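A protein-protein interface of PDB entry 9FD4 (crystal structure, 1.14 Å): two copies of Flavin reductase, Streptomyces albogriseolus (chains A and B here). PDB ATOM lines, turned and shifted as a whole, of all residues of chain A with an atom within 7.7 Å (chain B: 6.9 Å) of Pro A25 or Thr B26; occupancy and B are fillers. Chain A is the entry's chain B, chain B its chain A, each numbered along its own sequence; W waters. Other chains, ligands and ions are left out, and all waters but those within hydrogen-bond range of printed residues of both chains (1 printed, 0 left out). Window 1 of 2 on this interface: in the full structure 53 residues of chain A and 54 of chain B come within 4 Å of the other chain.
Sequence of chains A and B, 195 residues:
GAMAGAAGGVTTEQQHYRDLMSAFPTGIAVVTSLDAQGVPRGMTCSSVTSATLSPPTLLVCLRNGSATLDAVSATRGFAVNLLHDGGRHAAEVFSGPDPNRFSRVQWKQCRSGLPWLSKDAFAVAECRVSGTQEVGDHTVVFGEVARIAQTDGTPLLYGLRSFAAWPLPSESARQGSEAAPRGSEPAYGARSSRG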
ATOM      1  N   LEU A  20      -1.517 -10.512 -20.593  1.00  0.00           N
ATOM      2  CA  LEU A  20      -0.790  -9.542 -19.769  1.00  0.00           C
ATOM      3  C   LEU A  20       0.414 -10.191 -19.113  1.00  0.00           C
ATOM      4  O   LEU A  20       1.543  -9.701 -19.216  1.00  0.00           O
ATOM      5  CB  LEU A  20      -1.733  -9.016 -18.697  1.00  0.00           C
ATOM      6  CG  LEU A  20      -1.124  -8.126 -17.608  1.00  0.00           C
ATOM      7  CD1 LEU A  20      -0.835  -6.738 -18.131  1.00  0.00           C
ATOM      8  CD2 LEU A  20      -2.026  -8.123 -16.373  1.00  0.00           C
ATOM      9  N   MET A  21       0.189 -11.296 -18.412  1.00  0.00           N
ATOM     10  CA  MET A  21       1.261 -11.899 -17.638  1.00  0.00           C
ATOM     11  C   MET A  21       2.329 -12.508 -18.523  1.00  0.00           C
ATOM     12  O   MET A  21       3.502 -12.543 -18.152  1.00  0.00           O
ATOM     13  CB  MET A  21       0.679 -12.889 -16.621  1.00  0.00           C
ATOM     14  CG  MET A  21      -0.295 -12.272 -15.609  1.00  0.00           C
ATOM     15  SD  MET A  21       0.305 -10.848 -14.692  1.00  0.00           S
ATOM     16  CE  MET A  21       1.384 -11.661 -13.536  1.00  0.00           C
ATOM     17  N   SER A  22       1.953 -12.927 -19.720  1.00  0.00           N
ATOM     18  CA  SER A  22       2.943 -13.413 -20.659  1.00  0.00           C
ATOM     19  C   SER A  22       3.937 -12.335 -21.053  1.00  0.00           C
ATOM     20  O   SER A  22       5.039 -12.655 -21.510  1.00  0.00           O
ATOM     21  CB  SER A  22       2.224 -13.896 -21.910  1.00  0.00           C
ATOM     22  OG  SER A  22       3.151 -14.302 -22.887  1.00  0.00           O
ATOM     23  N   ALA A  23       3.562 -11.071 -20.921  1.00  0.00           N
ATOM     24  CA  ALA A  23       4.427  -9.957 -21.272  1.00  0.00           C
ATOM     25  C   ALA A  23       5.251  -9.426 -20.121  1.00  0.00           C
ATOM     26  O   ALA A  23       5.909  -8.387 -20.284  1.00  0.00           O
ATOM     27  CB  ALA A  23       3.605  -8.851 -21.927  1.00  0.00           C
ATOM     28  N   PHE A  24       5.265 -10.132 -18.991  1.00  0.00           N
ATOM     29  CA  PHE A  24       6.168  -9.863 -17.876  1.00  0.00           C
ATOM     30  C   PHE A  24       7.197 -10.990 -17.854  1.00  0.00           C
ATOM     31  O   PHE A  24       6.960 -12.048 -17.254  1.00  0.00           O
ATOM     32  CB  PHE A  24       5.392  -9.773 -16.550  1.00  0.00           C
ATOM     33  CG  PHE A  24       6.213  -9.300 -15.383  1.00  0.00           C
ATOM     34  CD1 PHE A  24       6.416  -7.951 -15.155  1.00  0.00           C
ATOM     35  CD2 PHE A  24       6.816 -10.236 -14.538  1.00  0.00           C
ATOM     36  CE1 PHE A  24       7.152  -7.549 -14.049  1.00  0.00           C
ATOM     37  CE2 PHE A  24       7.579  -9.848 -13.460  1.00  0.00           C
ATOM     38  CZ  PHE A  24       7.751  -8.510 -13.209  1.00  0.00           C
ATOM     39  N   PRO A  25       8.332 -10.847 -18.531  1.00  0.00           N
ATOM     40  CA  PRO A  25       9.282 -11.965 -18.590  1.00  0.00           C
ATOM     41  C   PRO A  25       9.944 -12.182 -17.239  1.00  0.00           C
ATOM     42  O   PRO A  25       9.994 -11.297 -16.380  1.00  0.00           O
ATOM     43  CB  PRO A  25      10.298 -11.524 -19.643  1.00  0.00           C
ATOM     44  CG  PRO A  25       9.559 -10.497 -20.470  1.00  0.00           C
ATOM     45  CD  PRO A  25       8.766  -9.744 -19.407  1.00  0.00           C
ATOM     46  N   THR A  26      10.474 -13.383 -17.067  1.00  0.00           N
ATOM     47  CA  THR A  26      11.123 -13.762 -15.826  1.00  0.00           C
ATOM     48  C   THR A  26      12.269 -14.726 -16.080  1.00  0.00           C
ATOM     49  O   THR A  26      12.373 -15.342 -17.141  1.00  0.00           O
ATOM     50  CB  THR A  26      10.172 -14.438 -14.826  1.00  0.00           C
ATOM     51  OG1 THR A  26       9.801 -15.720 -15.342  1.00  0.00           O
ATOM     52  CG2 THR A  26       8.904 -13.642 -14.533  1.00  0.00           C
ATOM     53  N   GLY A  27      13.094 -14.911 -15.058  1.00  0.00           N
ATOM     54  CA  GLY A  27      13.962 -16.059 -14.980  1.00  0.00           C
ATOM     55  C   GLY A  27      13.139 -17.339 -14.825  1.00  0.00           C
ATOM     56  O   GLY A  27      11.906 -17.345 -14.780  1.00  0.00           O
ATOM     57  N   SER A  46       8.202 -20.158 -12.663  1.00  0.00           N
ATOM     58  CA  SER A  46       8.577 -18.786 -12.932  1.00  0.00           C
ATOM     59  C   SER A  46       8.020 -17.811 -11.904  1.00  0.00           C
ATOM     60  O   SER A  46       8.258 -16.614 -12.036  1.00  0.00           O
ATOM     61  CB  SER A  46       8.166 -18.367 -14.328  1.00  0.00           C
ATOM     62  OG  SER A  46       6.768 -18.546 -14.483  1.00  0.00           O
ATOM     63  N   VAL A  48       8.944 -17.347  -8.790  1.00  0.00           N
ATOM     64  CA  VAL A  48       9.912 -16.975  -7.755  1.00  0.00           C
ATOM     65  C   VAL A  48       9.880 -15.468  -7.568  1.00  0.00           C
ATOM     66  O   VAL A  48      10.136 -14.729  -8.534  1.00  0.00           O
ATOM     67  CB  VAL A  48      11.326 -17.466  -8.131  1.00  0.00           C
ATOM     68  CG1 VAL A  48      12.321 -17.092  -7.019  1.00  0.00           C
ATOM     69  CG2 VAL A  48      11.380 -18.952  -8.377  1.00  0.00           C
ATOM     70  N   THR A  49       9.634 -15.014  -6.338  1.00  0.00           N
ATOM     71  CA  THR A  49       9.541 -13.606  -6.055  1.00  0.00           C
ATOM     72  C   THR A  49      10.172 -13.313  -4.711  1.00  0.00           C
ATOM     73  O   THR A  49       9.970 -14.038  -3.759  1.00  0.00           O
ATOM     74  CB  THR A  49       8.029 -13.287  -5.997  1.00  0.00           C
ATOM     75  OG1 THR A  49       7.426 -13.663  -7.242  1.00  0.00           O
ATOM     76  CG2 THR A  49       7.744 -11.872  -5.670  1.00  0.00           C
ATOM     77  N   LEU A 157      15.663 -17.134 -19.532  1.00  0.00           N
ATOM     78  CA  LEU A 157      14.434 -16.363 -19.393  1.00  0.00           C
ATOM     79  C   LEU A 157      13.280 -17.085 -20.068  1.00  0.00           C
ATOM     80  O   LEU A 157      13.473 -17.868 -21.003  1.00  0.00           O
ATOM     81  CB  LEU A 157      14.537 -14.985 -20.016  1.00  0.00           C
ATOM     82  CG  LEU A 157      15.678 -14.088 -19.599  1.00  0.00           C
ATOM     83  CD1 LEU A 157      15.668 -12.833 -20.439  1.00  0.00           C
ATOM     84  CD2 LEU A 157      15.580 -13.781 -18.118  1.00  0.00           C
ATOM     85  N   TYR A 158      12.068 -16.701 -19.652  1.00  0.00           N
ATOM     86  CA  TYR A 158      10.844 -17.047 -20.360  1.00  0.00           C
ATOM     87  C   TYR A 158       9.969 -15.824 -20.422  1.00  0.00           C
ATOM     88  O   TYR A 158       9.788 -15.140 -19.414  1.00  0.00           O
ATOM     89  CB  TYR A 158      10.105 -18.216 -19.697  1.00  0.00           C
ATOM     90  CG  TYR A 158       9.025 -18.844 -20.548  1.00  0.00           C
ATOM     91  CD1 TYR A 158       9.322 -19.878 -21.415  1.00  0.00           C
ATOM     92  CD2 TYR A 158       7.736 -18.407 -20.498  1.00  0.00           C
ATOM     93  CE1 TYR A 158       8.349 -20.437 -22.203  1.00  0.00           C
ATOM     94  CE2 TYR A 158       6.755 -18.966 -21.301  1.00  0.00           C
ATOM     95  CZ  TYR A 158       7.069 -19.991 -22.144  1.00  0.00           C
ATOM     96  OH  TYR A 158       6.124 -20.589 -22.955  1.00  0.00           O
ATOM     97  N   GLY A 159       9.425 -15.541 -21.603  1.00  0.00           N
ATOM     98  CA  GLY A 159       8.528 -14.414 -21.771  1.00  0.00           C
ATOM     99  C   GLY A 159       7.919 -14.437 -23.143  1.00  0.00           C
ATOM    100  O   GLY A 159       8.487 -14.997 -24.073  1.00  0.00           O
ATOM    101  N   LEU A 160       6.758 -13.810 -23.263  1.00  0.00           N
ATOM    102  CA  LEU A 160       6.078 -13.771 -24.549  1.00  0.00           C
ATOM    103  C   LEU A 160       6.072 -15.160 -25.185  1.00  0.00           C
ATOM    104  O   LEU A 160       6.348 -15.347 -26.378  1.00  0.00           O
ATOM    105  CB  LEU A 160       6.706 -12.726 -25.467  1.00  0.00           C
ATOM    106  CG  LEU A 160       6.544 -11.302 -24.926  1.00  0.00           C
ATOM    107  CD1 LEU A 160       7.335 -10.324 -25.780  1.00  0.00           C
ATOM    108  CD2 LEU A 160       5.067 -10.893 -24.848  1.00  0.00           C
ATOM    109  N   SER A 162       7.974 -17.690 -25.045  1.00  0.00           N
ATOM    110  CA  SER A 162       9.220 -18.206 -25.591  1.00  0.00           C
ATOM    111  C   SER A 162      10.297 -18.243 -24.521  1.00  0.00           C
ATOM    112  O   SER A 162      10.285 -17.461 -23.575  1.00  0.00           O
ATOM    113  CB  SER A 162       9.743 -17.322 -26.736  1.00  0.00           C
ATOM    114  OG  SER A 162      10.938 -17.848 -27.297  1.00  0.00           O
ATOM    115  N   ALA A 164      14.296 -17.489 -23.804  1.00  0.00           N
ATOM    116  CA  ALA A 164      15.354 -16.609 -24.261  1.00  0.00           C
ATOM    117  C   ALA A 164      16.458 -16.649 -23.216  1.00  0.00           C
ATOM    118  O   ALA A 164      16.399 -17.401 -22.239  1.00  0.00           O
ATOM    119  CB  ALA A 164      14.816 -15.200 -24.533  1.00  0.00           C
ATOM    120  N   TRP A 166      19.162 -14.004 -20.867  1.00  0.00           N
ATOM    121  CA  TRP A 166      19.525 -12.660 -20.461  1.00  0.00           C
ATOM    122  C   TRP A 166      20.501 -12.098 -21.490  1.00  0.00           C
ATOM    123  O   TRP A 166      21.474 -12.776 -21.842  1.00  0.00           O
ATOM    124  CB  TRP A 166      20.181 -12.717 -19.083  1.00  0.00           C
ATOM    125  CG  TRP A 166      20.601 -11.385 -18.585  1.00  0.00           C
ATOM    126  CD1 TRP A 166      21.871 -10.969 -18.423  1.00  0.00           C
ATOM    127  CD2 TRP A 166      19.760 -10.277 -18.232  1.00  0.00           C
ATOM    128  NE1 TRP A 166      21.898  -9.665 -17.992  1.00  0.00           N
ATOM    129  CE2 TRP A 166      20.611  -9.213 -17.871  1.00  0.00           C
ATOM    130  CE3 TRP A 166      18.374 -10.081 -18.175  1.00  0.00           C
ATOM    131  CZ2 TRP A 166      20.125  -7.978 -17.459  1.00  0.00           C
ATOM    132  CZ3 TRP A 166      17.900  -8.843 -17.784  1.00  0.00           C
ATOM    133  CH2 TRP A 166      18.773  -7.811 -17.445  1.00  0.00           C
ATOM    134  N   MET B  21      18.878 -13.127  -5.757  1.00  0.00           N
ATOM    135  CA  MET B  21      17.702 -12.598  -6.421  1.00  0.00           C
ATOM    136  C   MET B  21      18.044 -11.655  -7.567  1.00  0.00           C
ATOM    137  O   MET B  21      17.270 -11.540  -8.518  1.00  0.00           O
ATOM    138  CB  MET B  21      16.791 -11.963  -5.387  1.00  0.00           C
ATOM    139  CG  MET B  21      16.303 -12.940  -4.276  1.00  0.00           C
ATOM    140  SD  MET B  21      15.630 -14.517  -4.783  1.00  0.00           S
ATOM    141  CE  MET B  21      14.160 -13.935  -5.517  1.00  0.00           C
ATOM    142  N   SER B  22      19.195 -11.020  -7.499  1.00  0.00           N
ATOM    143  CA  SER B  22      19.631 -10.207  -8.616  1.00  0.00           C
ATOM    144  C   SER B  22      19.685 -11.041  -9.887  1.00  0.00           C
ATOM    145  O   SER B  22      19.416 -10.530 -10.987  1.00  0.00           O
ATOM    146  CB  SER B  22      21.004  -9.625  -8.297  1.00  0.00           C
ATOM    147  OG  SER B  22      21.501  -8.840  -9.357  1.00  0.00           O
ATOM    148  N   PHE B  24      17.762 -13.426 -10.877  1.00  0.00           N
ATOM    149  CA  PHE B  24      16.449 -13.800 -11.405  1.00  0.00           C
ATOM    150  C   PHE B  24      15.868 -12.562 -12.085  1.00  0.00           C
ATOM    151  O   PHE B  24      15.225 -11.724 -11.443  1.00  0.00           O
ATOM    152  CB  PHE B  24      15.527 -14.304 -10.280  1.00  0.00           C
ATOM    153  CG  PHE B  24      14.219 -14.902 -10.776  1.00  0.00           C
ATOM    154  CD1 PHE B  24      14.132 -16.226 -11.142  1.00  0.00           C
ATOM    155  CD2 PHE B  24      13.077 -14.123 -10.856  1.00  0.00           C
ATOM    156  CE1 PHE B  24      12.923 -16.765 -11.591  1.00  0.00           C
ATOM    157  CE2 PHE B  24      11.888 -14.644 -11.299  1.00  0.00           C
ATOM    158  CZ  PHE B  24      11.809 -15.962 -11.680  1.00  0.00           C
ATOM    159  N   PRO B  25      16.105 -12.358 -13.375  1.00  0.00           N
ATOM    160  CA  PRO B  25      15.624 -11.133 -14.026  1.00  0.00           C
ATOM    161  C   PRO B  25      14.114 -11.132 -14.179  1.00  0.00           C
ATOM    162  O   PRO B  25      13.458 -12.179 -14.162  1.00  0.00           O
ATOM    163  CB  PRO B  25      16.332 -11.155 -15.385  1.00  0.00           C
ATOM    164  CG  PRO B  25      17.475 -12.127 -15.225  1.00  0.00           C
ATOM    165  CD  PRO B  25      16.912 -13.168 -14.290  1.00  0.00           C
ATOM    166  N   THR B  26      13.566  -9.931 -14.345  1.00  0.00           N
ATOM    167  CA  THR B  26      12.136  -9.761 -14.501  1.00  0.00           C
ATOM    168  C   THR B  26      11.843  -8.596 -15.426  1.00  0.00           C
ATOM    169  O   THR B  26      12.684  -7.745 -15.697  1.00  0.00           O
ATOM    170  CB  THR B  26      11.439  -9.495 -13.169  1.00  0.00           C
ATOM    171  OG1 THR B  26      11.838  -8.225 -12.680  1.00  0.00           O
ATOM    172  CG2 THR B  26      11.705 -10.588 -12.141  1.00  0.00           C
ATOM    173  N   GLY B  27      10.596  -8.532 -15.853  1.00  0.00           N
ATOM    174  CA  GLY B  27      10.012  -7.314 -16.333  1.00  0.00           C
ATOM    175  C   GLY B  27       9.944  -6.240 -15.254  1.00  0.00           C
ATOM    176  O   GLY B  27      10.361  -6.456 -14.100  1.00  0.00           O
ATOM    177  N   ILE B  28       9.446  -5.064 -15.620  1.00  0.00           N
ATOM    178  CA  ILE B  28       9.392  -3.945 -14.689  1.00  0.00           C
ATOM    179  C   ILE B  28       8.036  -3.291 -14.759  1.00  0.00           C
ATOM    180  O   ILE B  28       7.625  -2.811 -15.816  1.00  0.00           O
ATOM    181  CB  ILE B  28      10.489  -2.900 -14.955  1.00  0.00           C
ATOM    182  CG1 ILE B  28      11.856  -3.489 -14.640  1.00  0.00           C
ATOM    183  CG2 ILE B  28      10.202  -1.631 -14.123  1.00  0.00           C
ATOM    184  CD1 ILE B  28      12.082  -3.717 -13.174  1.00  0.00           C
ATOM    185  N   ALA B  29       7.382  -3.181 -13.616  1.00  0.00           N
ATOM    186  CA  ALA B  29       6.149  -2.434 -13.491  1.00  0.00           C
ATOM    187  C   ALA B  29       6.380  -1.160 -12.700  1.00  0.00           C
ATOM    188  O   ALA B  29       7.305  -1.054 -11.894  1.00  0.00           O
ATOM    189  CB  ALA B  29       5.107  -3.269 -12.783  1.00  0.00           C
ATOM    190  N   CYS B  45       8.435  -1.666  -9.395  1.00  0.00           N
ATOM    191  CA  CYS B  45       8.103  -2.937  -8.771  1.00  0.00           C
ATOM    192  C   CYS B  45       8.491  -4.074  -9.711  1.00  0.00           C
ATOM    193  O   CYS B  45       7.974  -4.163 -10.831  1.00  0.00           O
ATOM    194  CB  CYS B  45       6.594  -2.972  -8.534  1.00  0.00           C
ATOM    195  SG  CYS B  45       5.983  -4.518  -7.791  1.00  0.00           S
ATOM    196  N   SER B  46       9.345  -4.989  -9.244  1.00  0.00           N
ATOM    197  CA  SER B  46       9.694  -6.189  -9.980  1.00  0.00           C
ATOM    198  C   SER B  46       9.069  -7.427  -9.377  1.00  0.00           C
ATOM    199  O   SER B  46       9.265  -8.499  -9.911  1.00  0.00           O
ATOM    200  CB  SER B  46      11.216  -6.369 -10.039  1.00  0.00           C
ATOM    201  OG  SER B  46      11.805  -6.390  -8.736  1.00  0.00           O
ATOM    202  N   SER B  47       8.259  -7.300  -8.322  1.00  0.00           N
ATOM    203  CA  SER B  47       7.665  -8.441  -7.614  1.00  0.00           C
ATOM    204  C   SER B  47       6.294  -8.888  -8.177  1.00  0.00           C
ATOM    205  O   SER B  47       5.563  -9.667  -7.537  1.00  0.00           O
ATOM    206  CB  SER B  47       7.572  -8.163  -6.121  1.00  0.00           C
ATOM    207  OG  SER B  47       6.765  -7.048  -5.871  1.00  0.00           O
ATOM    208  N   VAL B  48       5.920  -8.429  -9.354  1.00  0.00           N
ATOM    209  CA  VAL B  48       4.659  -8.858  -9.962  1.00  0.00           C
ATOM    210  C   VAL B  48       4.711 -10.358 -10.237  1.00  0.00           C
ATOM    211  O   VAL B  48       5.591 -10.835 -10.964  1.00  0.00           O
ATOM    212  CB  VAL B  48       4.433  -8.090 -11.277  1.00  0.00           C
ATOM    213  CG1 VAL B  48       3.100  -8.460 -11.911  1.00  0.00           C
ATOM    214  CG2 VAL B  48       4.495  -6.588 -11.068  1.00  0.00           C
ATOM    215  N   PHE B 122       3.383  -0.319 -21.865  1.00  0.00           N
ATOM    216  CA  PHE B 122       2.668  -0.948 -22.965  1.00  0.00           C
ATOM    217  C   PHE B 122       1.428  -1.695 -22.490  1.00  0.00           C
ATOM    218  O   PHE B 122       0.643  -2.141 -23.336  1.00  0.00           O
ATOM    219  CB  PHE B 122       3.573  -1.907 -23.770  1.00  0.00           C
ATOM    220  CG  PHE B 122       3.977  -3.139 -23.003  1.00  0.00           C
ATOM    221  CD1 PHE B 122       5.091  -3.158 -22.186  1.00  0.00           C
ATOM    222  CD2 PHE B 122       3.199  -4.274 -23.055  1.00  0.00           C
ATOM    223  CE1 PHE B 122       5.405  -4.287 -21.432  1.00  0.00           C
ATOM    224  CE2 PHE B 122       3.533  -5.410 -22.304  1.00  0.00           C
ATOM    225  CZ  PHE B 122       4.627  -5.400 -21.504  1.00  0.00           C
ATOM    226  N   PRO B 155       9.098  -5.562 -23.759  1.00  0.00           N
ATOM    227  CA  PRO B 155       9.235  -5.273 -22.320  1.00  0.00           C
ATOM    228  C   PRO B 155      10.630  -4.792 -21.936  1.00  0.00           C
ATOM    229  O   PRO B 155      11.644  -5.332 -22.392  1.00  0.00           O
ATOM    230  CB  PRO B 155       8.891  -6.610 -21.656  1.00  0.00           C
ATOM    231  CG  PRO B 155       8.056  -7.321 -22.658  1.00  0.00           C
ATOM    232  CD  PRO B 155       8.609  -6.938 -24.010  1.00  0.00           C
ATOM    233  N   LEU B 156      10.659  -3.819 -21.034  1.00  0.00           N
ATOM    234  CA  LEU B 156      11.858  -3.494 -20.267  1.00  0.00           C
ATOM    235  C   LEU B 156      12.156  -4.634 -19.293  1.00  0.00           C
ATOM    236  O   LEU B 156      11.239  -5.217 -18.722  1.00  0.00           O
ATOM    237  CB  LEU B 156      11.613  -2.181 -19.521  1.00  0.00           C
ATOM    238  CG  LEU B 156      12.790  -1.559 -18.780  1.00  0.00           C
ATOM    239  CD1 LEU B 156      13.895  -1.154 -19.761  1.00  0.00           C
ATOM    240  CD2 LEU B 156      12.319  -0.378 -17.951  1.00  0.00           C
ATOM    241  N   LEU B 157      13.419  -4.944 -19.090  1.00  0.00           N
ATOM    242  CA  LEU B 157      13.848  -5.911 -18.091  1.00  0.00           C
ATOM    243  C   LEU B 157      14.827  -5.284 -17.110  1.00  0.00           C
ATOM    244  O   LEU B 157      15.490  -4.282 -17.401  1.00  0.00           O
ATOM    245  CB  LEU B 157      14.567  -7.098 -18.711  1.00  0.00           C
ATOM    246  CG  LEU B 157      13.877  -7.839 -19.846  1.00  0.00           C
ATOM    247  CD1 LEU B 157      14.816  -8.890 -20.391  1.00  0.00           C
ATOM    248  CD2 LEU B 157      12.593  -8.456 -19.368  1.00  0.00           C
ATOM    249  N   TYR B 158      14.910  -5.916 -15.947  1.00  0.00           N
ATOM    250  CA  TYR B 158      15.949  -5.589 -14.983  1.00  0.00           C
ATOM    251  C   TYR B 158      16.509  -6.889 -14.433  1.00  0.00           C
ATOM    252  O   TYR B 158      15.751  -7.788 -14.062  1.00  0.00           O
ATOM    253  CB  TYR B 158      15.421  -4.736 -13.839  1.00  0.00           C
ATOM    254  CG  TYR B 158      16.498  -4.115 -13.005  1.00  0.00           C
ATOM    255  CD1 TYR B 158      17.099  -2.911 -13.373  1.00  0.00           C
ATOM    256  CD2 TYR B 158      16.922  -4.719 -11.841  1.00  0.00           C
ATOM    257  CE1 TYR B 158      18.085  -2.343 -12.607  1.00  0.00           C
ATOM    258  CE2 TYR B 158      17.916  -4.155 -11.060  1.00  0.00           C
ATOM    259  CZ  TYR B 158      18.490  -2.953 -11.445  1.00  0.00           C
ATOM    260  OH  TYR B 158      19.475  -2.367 -10.696  1.00  0.00           O
ATOM    261  N   GLY B 159      17.831  -6.977 -14.377  1.00  0.00           N
ATOM    262  CA  GLY B 159      18.480  -8.124 -13.784  1.00  0.00           C
ATOM    263  C   GLY B 159      19.968  -7.889 -13.746  1.00  0.00           C
ATOM    264  O   GLY B 159      20.498  -7.048 -14.478  1.00  0.00           O
ATOM    265  N   ALA B 164      17.777  -3.888 -19.239  1.00  0.00           N
ATOM    266  CA  ALA B 164      17.952  -4.433 -20.575  1.00  0.00           C
ATOM    267  C   ALA B 164      16.595  -4.443 -21.264  1.00  0.00           C
ATOM    268  O   ALA B 164      15.579  -4.115 -20.676  1.00  0.00           O
ATOM    269  CB  ALA B 164      18.577  -5.829 -20.516  1.00  0.00           C
ATOM    270  N   TRP B 166      13.896  -6.911 -23.487  1.00  0.00           N
ATOM    271  CA  TRP B 166      13.585  -8.267 -23.909  1.00  0.00           C
ATOM    272  C   TRP B 166      14.166  -8.511 -25.304  1.00  0.00           C
ATOM    273  O   TRP B 166      13.949  -7.688 -26.207  1.00  0.00           O
ATOM    274  CB  TRP B 166      12.068  -8.441 -23.937  1.00  0.00           C
ATOM    275  CG  TRP B 166      11.613  -9.709 -24.539  1.00  0.00           C
ATOM    276  CD1 TRP B 166      11.037  -9.858 -25.764  1.00  0.00           C
ATOM    277  CD2 TRP B 166      11.712 -11.014 -23.988  1.00  0.00           C
ATOM    278  NE1 TRP B 166      10.762 -11.163 -26.005  1.00  0.00           N
ATOM    279  CE2 TRP B 166      11.153 -11.895 -24.917  1.00  0.00           C
ATOM    280  CE3 TRP B 166      12.193 -11.523 -22.774  1.00  0.00           C
ATOM    281  CZ2 TRP B 166      11.095 -13.270 -24.698  1.00  0.00           C
ATOM    282  CZ3 TRP B 166      12.132 -12.886 -22.559  1.00  0.00           C
ATOM    283  CH2 TRP B 166      11.591 -13.743 -23.532  1.00  0.00           C
HETATM  284  O   HOH W   1      10.456 -11.608  -9.019  1.00  0.00           O
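The backbone carbonyl oxygen (O) of Pro B25 lies within hydrogen-bond range of the backbone NH (N) of Gly A27 (2.9 Å). The backbone NH (N) of Gly B27 lies within hydrogen-bond range of the backbone carbonyl oxygen (O) of Pro A25, at 2.9 Å.
O of Thr B26 is in hydrogen-bond range of N of Tyr B158. The side-chain sulfur of Cys B45 sits at hydrogen-bond distance from the side-chain hydroxyl of Ser B47, at 3.3 Å. The backbone carbonyl oxygen (O) of Pro B155 is in hydrogen-bond range of the backbone NH (N) of Trp B166, 3.0 Å away. N of Leu B157 is in hydrogen-bond range of O of Ala B164 (2.8 Å). O of Thr A26 lies within hydrogen-bond range of N of Tyr A158, at 2.9 Å. The backbone carbonyl oxygen (O) of Ala A164 sits at hydrogen-bond distance from the backbone NH (N) of Leu A157.
CE of Met A21 touches CG1 of Val B48 (3.98 Å). CB of Ala A23 touches CE2 of Phe B122, at 3.5 Å. N of Ile B28 touches CE1 of Phe A24, at 3.7 Å. Pro B155 touches Pro A25. Thr A26 touches Phe B24 (CB to CZ, 3.9 Å). CA of Thr A26 touches O of Pro B25 (3.3 Å). Leu A160 touches Trp B166. Ser A162 touches Trp B166. Trp A166 touches Pro B25. C of Tyr B158 touches CH2 of Trp A166 (3.9 Å).
Leu A20 touches none of the printed residues of chain B. Ser A22 touches none of the printed residues of chain B. Printed residues of chain B within 4 Å of Ala A23: Phe B122 and Pro B155. Printed residues of chain B within 4 Å of Pro A25: Thr B26 (3.2 Å), Gly B27 (2.9 Å), Pro B155 (3.9 Å), Leu B157 (3.8 Å) and Trp B166 (3.6 Å). Printed residues of chain B within 4 Å of Trp A166: Pro B25, Leu B157, Tyr B158, Gly B159 and Ala B164. Thr B26 touches two residues of chain A. Of the printed residues of chain A, Ala B164 touches Trp A166. The nearest residue of chain A that does not touch Thr B26 is Thr A26 (4.3 Å). The nearest printed residue of chain A that does not touch Trp B166 is Tyr A158 (4.1 Å).
Along chain B the printed residues that touch a printed residue of chain A span positions 21 to 166. Printed residues of chain A that touch a printed residue of chain B: Met A21, Ala A23, Phe A24, Pro A25, Thr A26, Gly A27, Ser A46, Val A48, Thr A49, Leu A157, Gly A159, Leu A160, Ser A162, Ala A164 and Trp A166. Hydrophobic or aromatic side chains of chain A within 4 Å of the printed part of chain B: Met A21, Ala A23, Phe A24, Pro A25, Val A48, Leu A157, Leu A160, Ala A164 and Trp A166. Among the printed residues, 31 pairs touch across the chains. Among the printed residues, no Asp or Glu carboxylate lies within 4 Å of a Lys or Arg side-chain nitrogen of the other chain.
Met A21 touches Val B48, and with the chains exchanged Val A48 touches Met B21. Phe A24 touches Val B48, and with the chains exchanged Val A48 touches Phe B24. Ala A164 touches Trp B166, and with the chains exchanged Trp A166 touches Ala B164. Trp A166 touches Leu B157, but with the chains exchanged Leu A157 does not touch Trp B166 (4.1 Å). Positions printed for both chains: 21, 22, 24, 25, 26, 27, 46, 48, 157, 158, 159, 164 and 166.
Water W1 lies within hydrogen-bond range of O of Val A48 (3.2 Å) and O of Ser B46 (3.4 Å).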
